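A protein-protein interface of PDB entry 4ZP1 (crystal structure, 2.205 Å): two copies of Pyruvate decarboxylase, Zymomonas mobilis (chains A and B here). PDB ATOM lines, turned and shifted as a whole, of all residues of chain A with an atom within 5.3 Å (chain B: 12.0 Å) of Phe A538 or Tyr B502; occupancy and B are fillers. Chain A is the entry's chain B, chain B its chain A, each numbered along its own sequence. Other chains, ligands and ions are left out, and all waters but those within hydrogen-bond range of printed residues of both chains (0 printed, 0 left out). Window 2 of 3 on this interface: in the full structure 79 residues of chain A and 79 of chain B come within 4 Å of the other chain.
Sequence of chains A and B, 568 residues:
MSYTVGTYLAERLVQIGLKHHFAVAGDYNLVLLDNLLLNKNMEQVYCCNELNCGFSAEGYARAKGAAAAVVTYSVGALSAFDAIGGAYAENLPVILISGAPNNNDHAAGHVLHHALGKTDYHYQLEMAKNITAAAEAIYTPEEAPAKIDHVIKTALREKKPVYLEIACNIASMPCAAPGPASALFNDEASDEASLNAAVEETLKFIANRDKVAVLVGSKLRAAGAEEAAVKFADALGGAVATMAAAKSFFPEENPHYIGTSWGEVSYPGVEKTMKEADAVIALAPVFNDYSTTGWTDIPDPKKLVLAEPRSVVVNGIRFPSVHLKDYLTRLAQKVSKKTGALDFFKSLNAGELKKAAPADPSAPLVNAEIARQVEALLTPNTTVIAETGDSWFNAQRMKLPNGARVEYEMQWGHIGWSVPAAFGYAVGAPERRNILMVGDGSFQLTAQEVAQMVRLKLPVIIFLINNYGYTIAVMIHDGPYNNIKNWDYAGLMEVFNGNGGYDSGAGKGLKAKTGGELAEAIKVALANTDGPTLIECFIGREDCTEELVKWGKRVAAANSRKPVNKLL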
ATOM      1  N   LEU A 365     -25.000   0.644  -9.227  1.00  0.00           N
ATOM      2  CA  LEU A 365     -24.628   0.526 -10.630  1.00  0.00           C
ATOM      3  C   LEU A 365     -25.208  -0.729 -11.275  1.00  0.00           C
ATOM      4  O   LEU A 365     -25.209  -1.804 -10.675  1.00  0.00           O
ATOM      5  CB  LEU A 365     -23.106   0.526 -10.766  1.00  0.00           C
ATOM      6  CG  LEU A 365     -22.558   0.374 -12.182  1.00  0.00           C
ATOM      7  CD1 LEU A 365     -22.979   1.554 -13.051  1.00  0.00           C
ATOM      8  CD2 LEU A 365     -21.043   0.236 -12.135  1.00  0.00           C
ATOM      9  N   ASN A 466     -16.725  -6.298 -12.613  1.00  0.00           N
ATOM     10  CA  ASN A 466     -16.733  -7.205 -11.476  1.00  0.00           C
ATOM     11  C   ASN A 466     -18.141  -7.676 -11.103  1.00  0.00           C
ATOM     12  O   ASN A 466     -18.836  -7.026 -10.316  1.00  0.00           O
ATOM     13  CB  ASN A 466     -16.077  -6.538 -10.266  1.00  0.00           C
ATOM     14  CG  ASN A 466     -15.625  -7.545  -9.227  1.00  0.00           C
ATOM     15  OD1 ASN A 466     -15.985  -8.715  -9.297  1.00  0.00           O
ATOM     16  ND2 ASN A 466     -14.837  -7.094  -8.259  1.00  0.00           N
ATOM     17  N   ASN A 467     -18.560  -8.805 -11.670  1.00  0.00           N
ATOM     18  CA  ASN A 467     -19.803  -9.447 -11.254  1.00  0.00           C
ATOM     19  C   ASN A 467     -19.527 -10.743 -10.486  1.00  0.00           C
ATOM     20  O   ASN A 467     -20.426 -11.560 -10.277  1.00  0.00           O
ATOM     21  CB  ASN A 467     -20.701  -9.727 -12.460  1.00  0.00           C
ATOM     22  CG  ASN A 467     -20.027 -10.597 -13.497  1.00  0.00           C
ATOM     23  OD1 ASN A 467     -18.894 -11.041 -13.312  1.00  0.00           O
ATOM     24  ND2 ASN A 467     -20.725 -10.857 -14.595  1.00  0.00           N
ATOM     25  N   TYR A 468     -18.270 -10.926 -10.088  1.00  0.00           N
ATOM     26  CA  TYR A 468     -17.858 -12.045  -9.239  1.00  0.00           C
ATOM     27  C   TYR A 468     -18.087 -13.416  -9.878  1.00  0.00           C
ATOM     28  O   TYR A 468     -18.846 -14.230  -9.350  1.00  0.00           O
ATOM     29  CB  TYR A 468     -18.594 -11.979  -7.897  1.00  0.00           C
ATOM     30  CG  TYR A 468     -17.949 -12.781  -6.786  1.00  0.00           C
ATOM     31  CD1 TYR A 468     -16.596 -13.089  -6.820  1.00  0.00           C
ATOM     32  CD2 TYR A 468     -18.696 -13.232  -5.703  1.00  0.00           C
ATOM     33  CE1 TYR A 468     -16.003 -13.816  -5.805  1.00  0.00           C
ATOM     34  CE2 TYR A 468     -18.112 -13.965  -4.683  1.00  0.00           C
ATOM     35  CZ  TYR A 468     -16.765 -14.255  -4.741  1.00  0.00           C
ATOM     36  OH  TYR A 468     -16.174 -14.983  -3.732  1.00  0.00           O
ATOM     37  N   ASN A 486     -12.392 -13.371  -5.684  1.00  0.00           N
ATOM     38  CA  ASN A 486     -12.471 -11.943  -5.953  1.00  0.00           C
ATOM     39  C   ASN A 486     -11.177 -11.242  -5.543  1.00  0.00           C
ATOM     40  O   ASN A 486     -10.614 -11.542  -4.487  1.00  0.00           O
ATOM     41  CB  ASN A 486     -13.669 -11.329  -5.223  1.00  0.00           C
ATOM     42  CG  ASN A 486     -13.911  -9.870  -5.609  1.00  0.00           C
ATOM     43  OD1 ASN A 486     -14.371  -9.576  -6.712  1.00  0.00           O
ATOM     44  ND2 ASN A 486     -13.620  -8.954  -4.689  1.00  0.00           N
ATOM     45  N   LYS A 511     -12.617   2.750  -8.037  1.00  0.00           N
ATOM     46  CA  LYS A 511     -13.791   1.902  -7.869  1.00  0.00           C
ATOM     47  C   LYS A 511     -15.062   2.670  -8.225  1.00  0.00           C
ATOM     48  O   LYS A 511     -15.186   3.862  -7.927  1.00  0.00           O
ATOM     49  CB  LYS A 511     -13.884   1.365  -6.433  1.00  0.00           C
ATOM     50  CG  LYS A 511     -12.744   0.443  -6.014  1.00  0.00           C
ATOM     51  CD  LYS A 511     -12.915  -0.021  -4.570  1.00  0.00           C
ATOM     52  CE  LYS A 511     -11.776  -0.925  -4.112  1.00  0.00           C
ATOM     53  NZ  LYS A 511     -11.762  -2.260  -4.789  1.00  0.00           N
ATOM     54  N   ALA A 512     -16.003   1.984  -8.864  1.00  0.00           N
ATOM     55  CA  ALA A 512     -17.292   2.585  -9.194  1.00  0.00           C
ATOM     56  C   ALA A 512     -18.436   1.645  -8.820  1.00  0.00           C
ATOM     57  O   ALA A 512     -18.539   0.531  -9.339  1.00  0.00           O
ATOM     58  CB  ALA A 512     -17.353   2.943 -10.667  1.00  0.00           C
ATOM     59  N   LYS A 513     -19.292   2.108  -7.913  1.00  0.00           N
ATOM     60  CA  LYS A 513     -20.416   1.319  -7.422  1.00  0.00           C
ATOM     61  C   LYS A 513     -21.745   1.976  -7.771  1.00  0.00           C
ATOM     62  O   LYS A 513     -22.791   1.329  -7.751  1.00  0.00           O
ATOM     63  CB  LYS A 513     -20.310   1.124  -5.910  1.00  0.00           C
ATOM     64  CG  LYS A 513     -18.988   0.529  -5.460  1.00  0.00           C
ATOM     65  CD  LYS A 513     -19.010   0.189  -3.983  1.00  0.00           C
ATOM     66  CE  LYS A 513     -17.773  -0.598  -3.589  1.00  0.00           C
ATOM     67  NZ  LYS A 513     -17.903  -1.167  -2.219  1.00  0.00           N
ATOM     68  N   GLU A 536     -12.895  -0.285 -11.778  1.00  0.00           N
ATOM     69  CA  GLU A 536     -13.544  -1.501 -11.314  1.00  0.00           C
ATOM     70  C   GLU A 536     -15.020  -1.232 -11.038  1.00  0.00           C
ATOM     71  O   GLU A 536     -15.366  -0.529 -10.088  1.00  0.00           O
ATOM     72  CB  GLU A 536     -12.850  -2.045 -10.061  1.00  0.00           C
ATOM     73  CG  GLU A 536     -13.546  -3.253  -9.445  1.00  0.00           C
ATOM     74  CD  GLU A 536     -12.857  -3.760  -8.189  1.00  0.00           C
ATOM     75  OE1 GLU A 536     -11.844  -3.163  -7.771  1.00  0.00           O
ATOM     76  OE2 GLU A 536     -13.331  -4.762  -7.614  1.00  0.00           O
ATOM     77  N   CYS A 537     -15.882  -1.794 -11.881  1.00  0.00           N
ATOM     78  CA  CYS A 537     -17.323  -1.586 -11.778  1.00  0.00           C
ATOM     79  C   CYS A 537     -18.016  -2.767 -11.120  1.00  0.00           C
ATOM     80  O   CYS A 537     -17.899  -3.895 -11.592  1.00  0.00           O
ATOM     81  CB  CYS A 537     -17.926  -1.349 -13.161  1.00  0.00           C
ATOM     82  SG  CYS A 537     -17.050  -0.137 -14.141  1.00  0.00           S
ATOM     83  N   PHE A 538     -18.750  -2.506 -10.042  1.00  0.00           N
ATOM     84  CA  PHE A 538     -19.456  -3.564  -9.324  1.00  0.00           C
ATOM     85  C   PHE A 538     -20.911  -3.709  -9.765  1.00  0.00           C
ATOM     86  O   PHE A 538     -21.686  -2.756  -9.707  1.00  0.00           O
ATOM     87  CB  PHE A 538     -19.419  -3.309  -7.818  1.00  0.00           C
ATOM     88  CG  PHE A 538     -18.043  -3.327  -7.230  1.00  0.00           C
ATOM     89  CD1 PHE A 538     -17.220  -2.212  -7.325  1.00  0.00           C
ATOM     90  CD2 PHE A 538     -17.577  -4.452  -6.561  1.00  0.00           C
ATOM     91  CE1 PHE A 538     -15.952  -2.223  -6.773  1.00  0.00           C
ATOM     92  CE2 PHE A 538     -16.312  -4.473  -6.006  1.00  0.00           C
ATOM     93  CZ  PHE A 538     -15.497  -3.361  -6.107  1.00  0.00           C
ATOM     94  N   ILE A 539     -21.271  -4.913 -10.191  1.00  0.00           N
ATOM     95  CA  ILE A 539     -22.654  -5.248 -10.512  1.00  0.00           C
ATOM     96  C   ILE A 539     -22.954  -6.692 -10.097  1.00  0.00           C
ATOM     97  O   ILE A 539     -22.039  -7.469  -9.838  1.00  0.00           O
ATOM     98  CB  ILE A 539     -22.947  -5.066 -12.008  1.00  0.00           C
ATOM     99  CG1 ILE A 539     -22.031  -5.966 -12.837  1.00  0.00           C
ATOM    100  CG2 ILE A 539     -22.761  -3.621 -12.407  1.00  0.00           C
ATOM    101  CD1 ILE A 539     -22.279  -5.885 -14.319  1.00  0.00           C
ATOM    102  N   GLY A 540     -24.235  -7.044 -10.034  1.00  0.00           N
ATOM    103  CA  GLY A 540     -24.644  -8.387  -9.655  1.00  0.00           C
ATOM    104  C   GLY A 540     -24.354  -9.416 -10.732  1.00  0.00           C
ATOM    105  O   GLY A 540     -24.135  -9.067 -11.893  1.00  0.00           O
ATOM    106  N   VAL B 454      -4.418 -18.200  -1.250  1.00  0.00           N
ATOM    107  CA  VAL B 454      -5.266 -17.432  -0.347  1.00  0.00           C
ATOM    108  C   VAL B 454      -6.630 -18.094  -0.213  1.00  0.00           C
ATOM    109  O   VAL B 454      -7.140 -18.282   0.888  1.00  0.00           O
ATOM    110  CB  VAL B 454      -5.473 -15.970  -0.837  1.00  0.00           C
ATOM    111  CG1 VAL B 454      -6.426 -15.234   0.085  1.00  0.00           C
ATOM    112  CG2 VAL B 454      -4.144 -15.224  -0.941  1.00  0.00           C
ATOM    113  N   ARG B 455      -7.207 -18.438  -1.357  1.00  0.00           N
ATOM    114  CA  ARG B 455      -8.534 -19.033  -1.439  1.00  0.00           C
ATOM    115  C   ARG B 455      -8.656 -20.313  -0.604  1.00  0.00           C
ATOM    116  O   ARG B 455      -9.654 -20.527   0.082  1.00  0.00           O
ATOM    117  CB  ARG B 455      -8.856 -19.319  -2.905  1.00  0.00           C
ATOM    118  CG  ARG B 455     -10.298 -19.667  -3.219  1.00  0.00           C
ATOM    119  CD  ARG B 455     -10.401 -19.966  -4.709  1.00  0.00           C
ATOM    120  NE  ARG B 455     -11.759 -20.250  -5.161  1.00  0.00           N
ATOM    121  CZ  ARG B 455     -12.088 -20.443  -6.436  1.00  0.00           C
ATOM    122  NH1 ARG B 455     -11.158 -20.374  -7.383  1.00  0.00           N
ATOM    123  NH2 ARG B 455     -13.347 -20.702  -6.766  1.00  0.00           N
ATOM    124  N   GLU B 494      -2.686  -8.169  -0.336  1.00  0.00           N
ATOM    125  CA  GLU B 494      -3.961  -7.550   0.029  1.00  0.00           C
ATOM    126  C   GLU B 494      -4.866  -7.457  -1.193  1.00  0.00           C
ATOM    127  O   GLU B 494      -6.081  -7.587  -1.086  1.00  0.00           O
ATOM    128  CB  GLU B 494      -3.754  -6.167   0.654  1.00  0.00           C
ATOM    129  CG  GLU B 494      -3.268  -6.212   2.099  1.00  0.00           C
ATOM    130  CD  GLU B 494      -4.171  -7.040   3.002  1.00  0.00           C
ATOM    131  OE1 GLU B 494      -5.387  -7.119   2.724  1.00  0.00           O
ATOM    132  OE2 GLU B 494      -3.665  -7.618   3.987  1.00  0.00           O
ATOM    133  N   VAL B 495      -4.268  -7.242  -2.357  1.00  0.00           N
ATOM    134  CA  VAL B 495      -5.024  -7.305  -3.597  1.00  0.00           C
ATOM    135  C   VAL B 495      -5.708  -8.666  -3.743  1.00  0.00           C
ATOM    136  O   VAL B 495      -6.895  -8.742  -4.062  1.00  0.00           O
ATOM    137  CB  VAL B 495      -4.133  -7.057  -4.815  1.00  0.00           C
ATOM    138  CG1 VAL B 495      -4.872  -7.439  -6.088  1.00  0.00           C
ATOM    139  CG2 VAL B 495      -3.690  -5.598  -4.855  1.00  0.00           C
ATOM    140  N   PHE B 496      -4.970  -9.743  -3.494  1.00  0.00           N
ATOM    141  CA  PHE B 496      -5.554 -11.074  -3.635  1.00  0.00           C
ATOM    142  C   PHE B 496      -6.505 -11.406  -2.483  1.00  0.00           C
ATOM    143  O   PHE B 496      -7.402 -12.235  -2.637  1.00  0.00           O
ATOM    144  CB  PHE B 496      -4.452 -12.129  -3.757  1.00  0.00           C
ATOM    145  CG  PHE B 496      -3.677 -12.042  -5.051  1.00  0.00           C
ATOM    146  CD1 PHE B 496      -4.262 -11.499  -6.188  1.00  0.00           C
ATOM    147  CD2 PHE B 496      -2.367 -12.486  -5.125  1.00  0.00           C
ATOM    148  CE1 PHE B 496      -3.558 -11.413  -7.370  1.00  0.00           C
ATOM    149  CE2 PHE B 496      -1.657 -12.403  -6.309  1.00  0.00           C
ATOM    150  CZ  PHE B 496      -2.250 -11.868  -7.430  1.00  0.00           C
ATOM    151  N   ASN B 497      -6.323 -10.754  -1.337  1.00  0.00           N
ATOM    152  CA  ASN B 497      -7.251 -10.934  -0.224  1.00  0.00           C
ATOM    153  C   ASN B 497      -8.625 -10.378  -0.572  1.00  0.00           C
ATOM    154  O   ASN B 497      -9.648 -11.003  -0.295  1.00  0.00           O
ATOM    155  CB  ASN B 497      -6.726 -10.263   1.051  1.00  0.00           C
ATOM    156  CG  ASN B 497      -5.682 -11.104   1.777  1.00  0.00           C
ATOM    157  OD1 ASN B 497      -5.571 -12.307   1.554  1.00  0.00           O
ATOM    158  ND2 ASN B 497      -4.917 -10.467   2.661  1.00  0.00           N
ATOM    159  N   GLY B 498      -8.635  -9.197  -1.184  1.00  0.00           N
ATOM    160  CA  GLY B 498      -9.866  -8.511  -1.533  1.00  0.00           C
ATOM    161  C   GLY B 498     -10.703  -8.175  -0.315  1.00  0.00           C
ATOM    162  O   GLY B 498     -11.932  -8.228  -0.366  1.00  0.00           O
ATOM    163  N   ASN B 499     -10.040  -7.838   0.787  1.00  0.00           N
ATOM    164  CA  ASN B 499     -10.748  -7.576   2.032  1.00  0.00           C
ATOM    165  C   ASN B 499     -11.570  -6.303   1.941  1.00  0.00           C
ATOM    166  O   ASN B 499     -11.038  -5.219   1.694  1.00  0.00           O
ATOM    167  CB  ASN B 499      -9.770  -7.510   3.204  1.00  0.00           C
ATOM    168  CG  ASN B 499      -9.220  -8.876   3.574  1.00  0.00           C
ATOM    169  OD1 ASN B 499      -9.951  -9.871   3.582  1.00  0.00           O
ATOM    170  ND2 ASN B 499      -7.926  -8.936   3.865  1.00  0.00           N
ATOM    171  N   GLY B 500     -12.877  -6.451   2.133  1.00  0.00           N
ATOM    172  CA  GLY B 500     -13.816  -5.364   1.929  1.00  0.00           C
ATOM    173  C   GLY B 500     -14.655  -5.612   0.690  1.00  0.00           C
ATOM    174  O   GLY B 500     -15.532  -4.821   0.351  1.00  0.00           O
ATOM    175  N   GLY B 501     -14.385  -6.726   0.014  1.00  0.00           N
ATOM    176  CA  GLY B 501     -15.084  -7.071  -1.211  1.00  0.00           C
ATOM    177  C   GLY B 501     -16.080  -8.208  -1.057  1.00  0.00           C
ATOM    178  O   GLY B 501     -16.664  -8.396   0.011  1.00  0.00           O
ATOM    179  N   TYR B 502     -16.267  -8.967  -2.133  1.00  0.00           N
ATOM    180  CA  TYR B 502     -17.236 -10.062  -2.163  1.00  0.00           C
ATOM    181  C   TYR B 502     -16.873 -11.216  -1.227  1.00  0.00           C
ATOM    182  O   TYR B 502     -17.745 -11.796  -0.582  1.00  0.00           O
ATOM    183  CB  TYR B 502     -17.387 -10.588  -3.593  1.00  0.00           C
ATOM    184  CG  TYR B 502     -18.060  -9.615  -4.535  1.00  0.00           C
ATOM    185  CD1 TYR B 502     -19.098  -8.802  -4.100  1.00  0.00           C
ATOM    186  CD2 TYR B 502     -17.655  -9.507  -5.859  1.00  0.00           C
ATOM    187  CE1 TYR B 502     -19.716  -7.910  -4.957  1.00  0.00           C
ATOM    188  CE2 TYR B 502     -18.268  -8.619  -6.725  1.00  0.00           C
ATOM    189  CZ  TYR B 502     -19.297  -7.824  -6.268  1.00  0.00           C
ATOM    190  OH  TYR B 502     -19.907  -6.935  -7.123  1.00  0.00           O
ATOM    191  N   ASP B 503     -15.588 -11.554  -1.161  1.00  0.00           N
ATOM    192  CA  ASP B 503     -15.120 -12.591  -0.242  1.00  0.00           C
ATOM    193  C   ASP B 503     -13.993 -12.056   0.636  1.00  0.00           C
ATOM    194  O   ASP B 503     -13.891 -10.845   0.847  1.00  0.00           O
ATOM    195  CB  ASP B 503     -14.662 -13.840  -1.006  1.00  0.00           C
ATOM    196  CG  ASP B 503     -13.719 -13.518  -2.157  1.00  0.00           C
ATOM    197  OD1 ASP B 503     -12.978 -12.517  -2.071  1.00  0.00           O
ATOM    198  OD2 ASP B 503     -13.719 -14.275  -3.152  1.00  0.00           O
ATOM    199  N   SER B 504     -13.150 -12.951   1.145  1.00  0.00           N
ATOM    200  CA  SER B 504     -12.047 -12.532   2.001  1.00  0.00           C
ATOM    201  C   SER B 504     -10.779 -13.330   1.741  1.00  0.00           C
ATOM    202  O   SER B 504     -10.766 -14.247   0.920  1.00  0.00           O
ATOM    203  CB  SER B 504     -12.435 -12.658   3.471  1.00  0.00           C
ATOM    204  OG  SER B 504     -12.540 -14.020   3.840  1.00  0.00           O
ATOM    205  N   GLY B 505      -9.716 -12.970   2.453  1.00  0.00           N
ATOM    206  CA  GLY B 505      -8.438 -13.651   2.348  1.00  0.00           C
ATOM    207  C   GLY B 505      -7.609 -13.370   3.586  1.00  0.00           C
ATOM    208  O   GLY B 505      -7.783 -12.332   4.229  1.00  0.00           O
ATOM    209  N   ALA B 506      -6.712 -14.289   3.928  1.00  0.00           N
ATOM    210  CA  ALA B 506      -5.893 -14.134   5.124  1.00  0.00           C
ATOM    211  C   ALA B 506      -4.398 -14.110   4.802  1.00  0.00           C
ATOM    212  O   ALA B 506      -3.563 -14.314   5.683  1.00  0.00           O
ATOM    213  CB  ALA B 506      -6.198 -15.244   6.117  1.00  0.00           C
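OH of Tyr B502 lies within hydrogen-bond range of O of Ile A539 (3.5 Å). The side-chain carboxylate (OD2) of Asp B503 sits at hydrogen-bond distance from the side-chain hydroxyl (OH) of Tyr A468, at 2.6 Å. The side-chain hydroxyl (OH) of Tyr B502 is in hydrogen-bond range of the backbone carbonyl oxygen (O) of Asn A466 (3.4 Å). The side-chain carboxylate of Asp B503 sits at hydrogen-bond distance from the backbone NH of Asn A486, at 3.0 Å.
The backbone carbonyl oxygen (O) of Asn A466 lies within hydrogen-bond range of the backbone NH (N) of Ile A539 (3.2 Å). OD1 of Asn A486 lies within hydrogen-bond range of ND2 of Asn A466, at 3.0 Å. The side-chain amide nitrogen of Asn A466 lies within hydrogen-bond range of the side-chain carboxylate of Glu A536, at 2.8 Å. N of Phe A538 sits at hydrogen-bond distance from O of Ala A512. The side-chain amide oxygen (OD1) of Asn A466 lies within hydrogen-bond range of the backbone NH (N) of Tyr A468. N of Asn A466 sits at hydrogen-bond distance from O of Cys A537 (2.9 Å).
Among the printed residues, pairs that only touch across the chains: Tyr A468 with Tyr B502 (3.3 Å), Asn A486 with Tyr B502 (3.4 Å), Phe A538 with Tyr B502 (3.5 Å) and Asn A486 with Phe B496 (3.8 Å).
Of chain A, only Asn A466 (3.4 Å), Tyr A468 (3.3 Å), Asn A486 (3.4 Å), Phe A538 (3.5 Å) and Ile A539 (3.5 Å) come within 4 Å of Tyr B502. Of the printed residues of chain B, Asn A466 touches Tyr B502. Asn A486 touches just these residues of chain B: Phe B496 (3.8 Å), Tyr B502 (3.4 Å) and Asp B503 (3.0 Å). No residue of chain B comes within 4 Å of Lys A511. Ala A512 touches none of the printed residues of chain B. No residue of chain B comes within 4 Å of Lys A513. No residue of chain B comes within 4 Å of Glu A536. No residue of chain B comes within 4 Å of Cys A537. Printed residues of chain A within 4 Å of Phe B496: Asn A486 (3.8 Å). Of the printed residues of chain A, Asp B503 touches Tyr A468 and Asn A486. Val B495 touches none of the printed residues of chain A. Ala B506 touches none of the printed residues of chain A. The nearest residue of chain B that does not touch Phe A538 is Gly B501 (5.6 Å).
Hydrophobic or aromatic side chains of chain A within 4 Å of the printed part of chain B: Tyr A468 and Phe A538. Of the 15 printed residues of chain B, 3 touch a printed residue of chain A. Hydrophobic or aromatic side chains of chain B within 4 Å of the printed part of chain A: Tyr B502. Among the printed residues, no Asp or Glu carboxylate lies within 4 Å of a Lys or Arg side-chain nitrogen of the other chain.
No position is printed for both chains.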
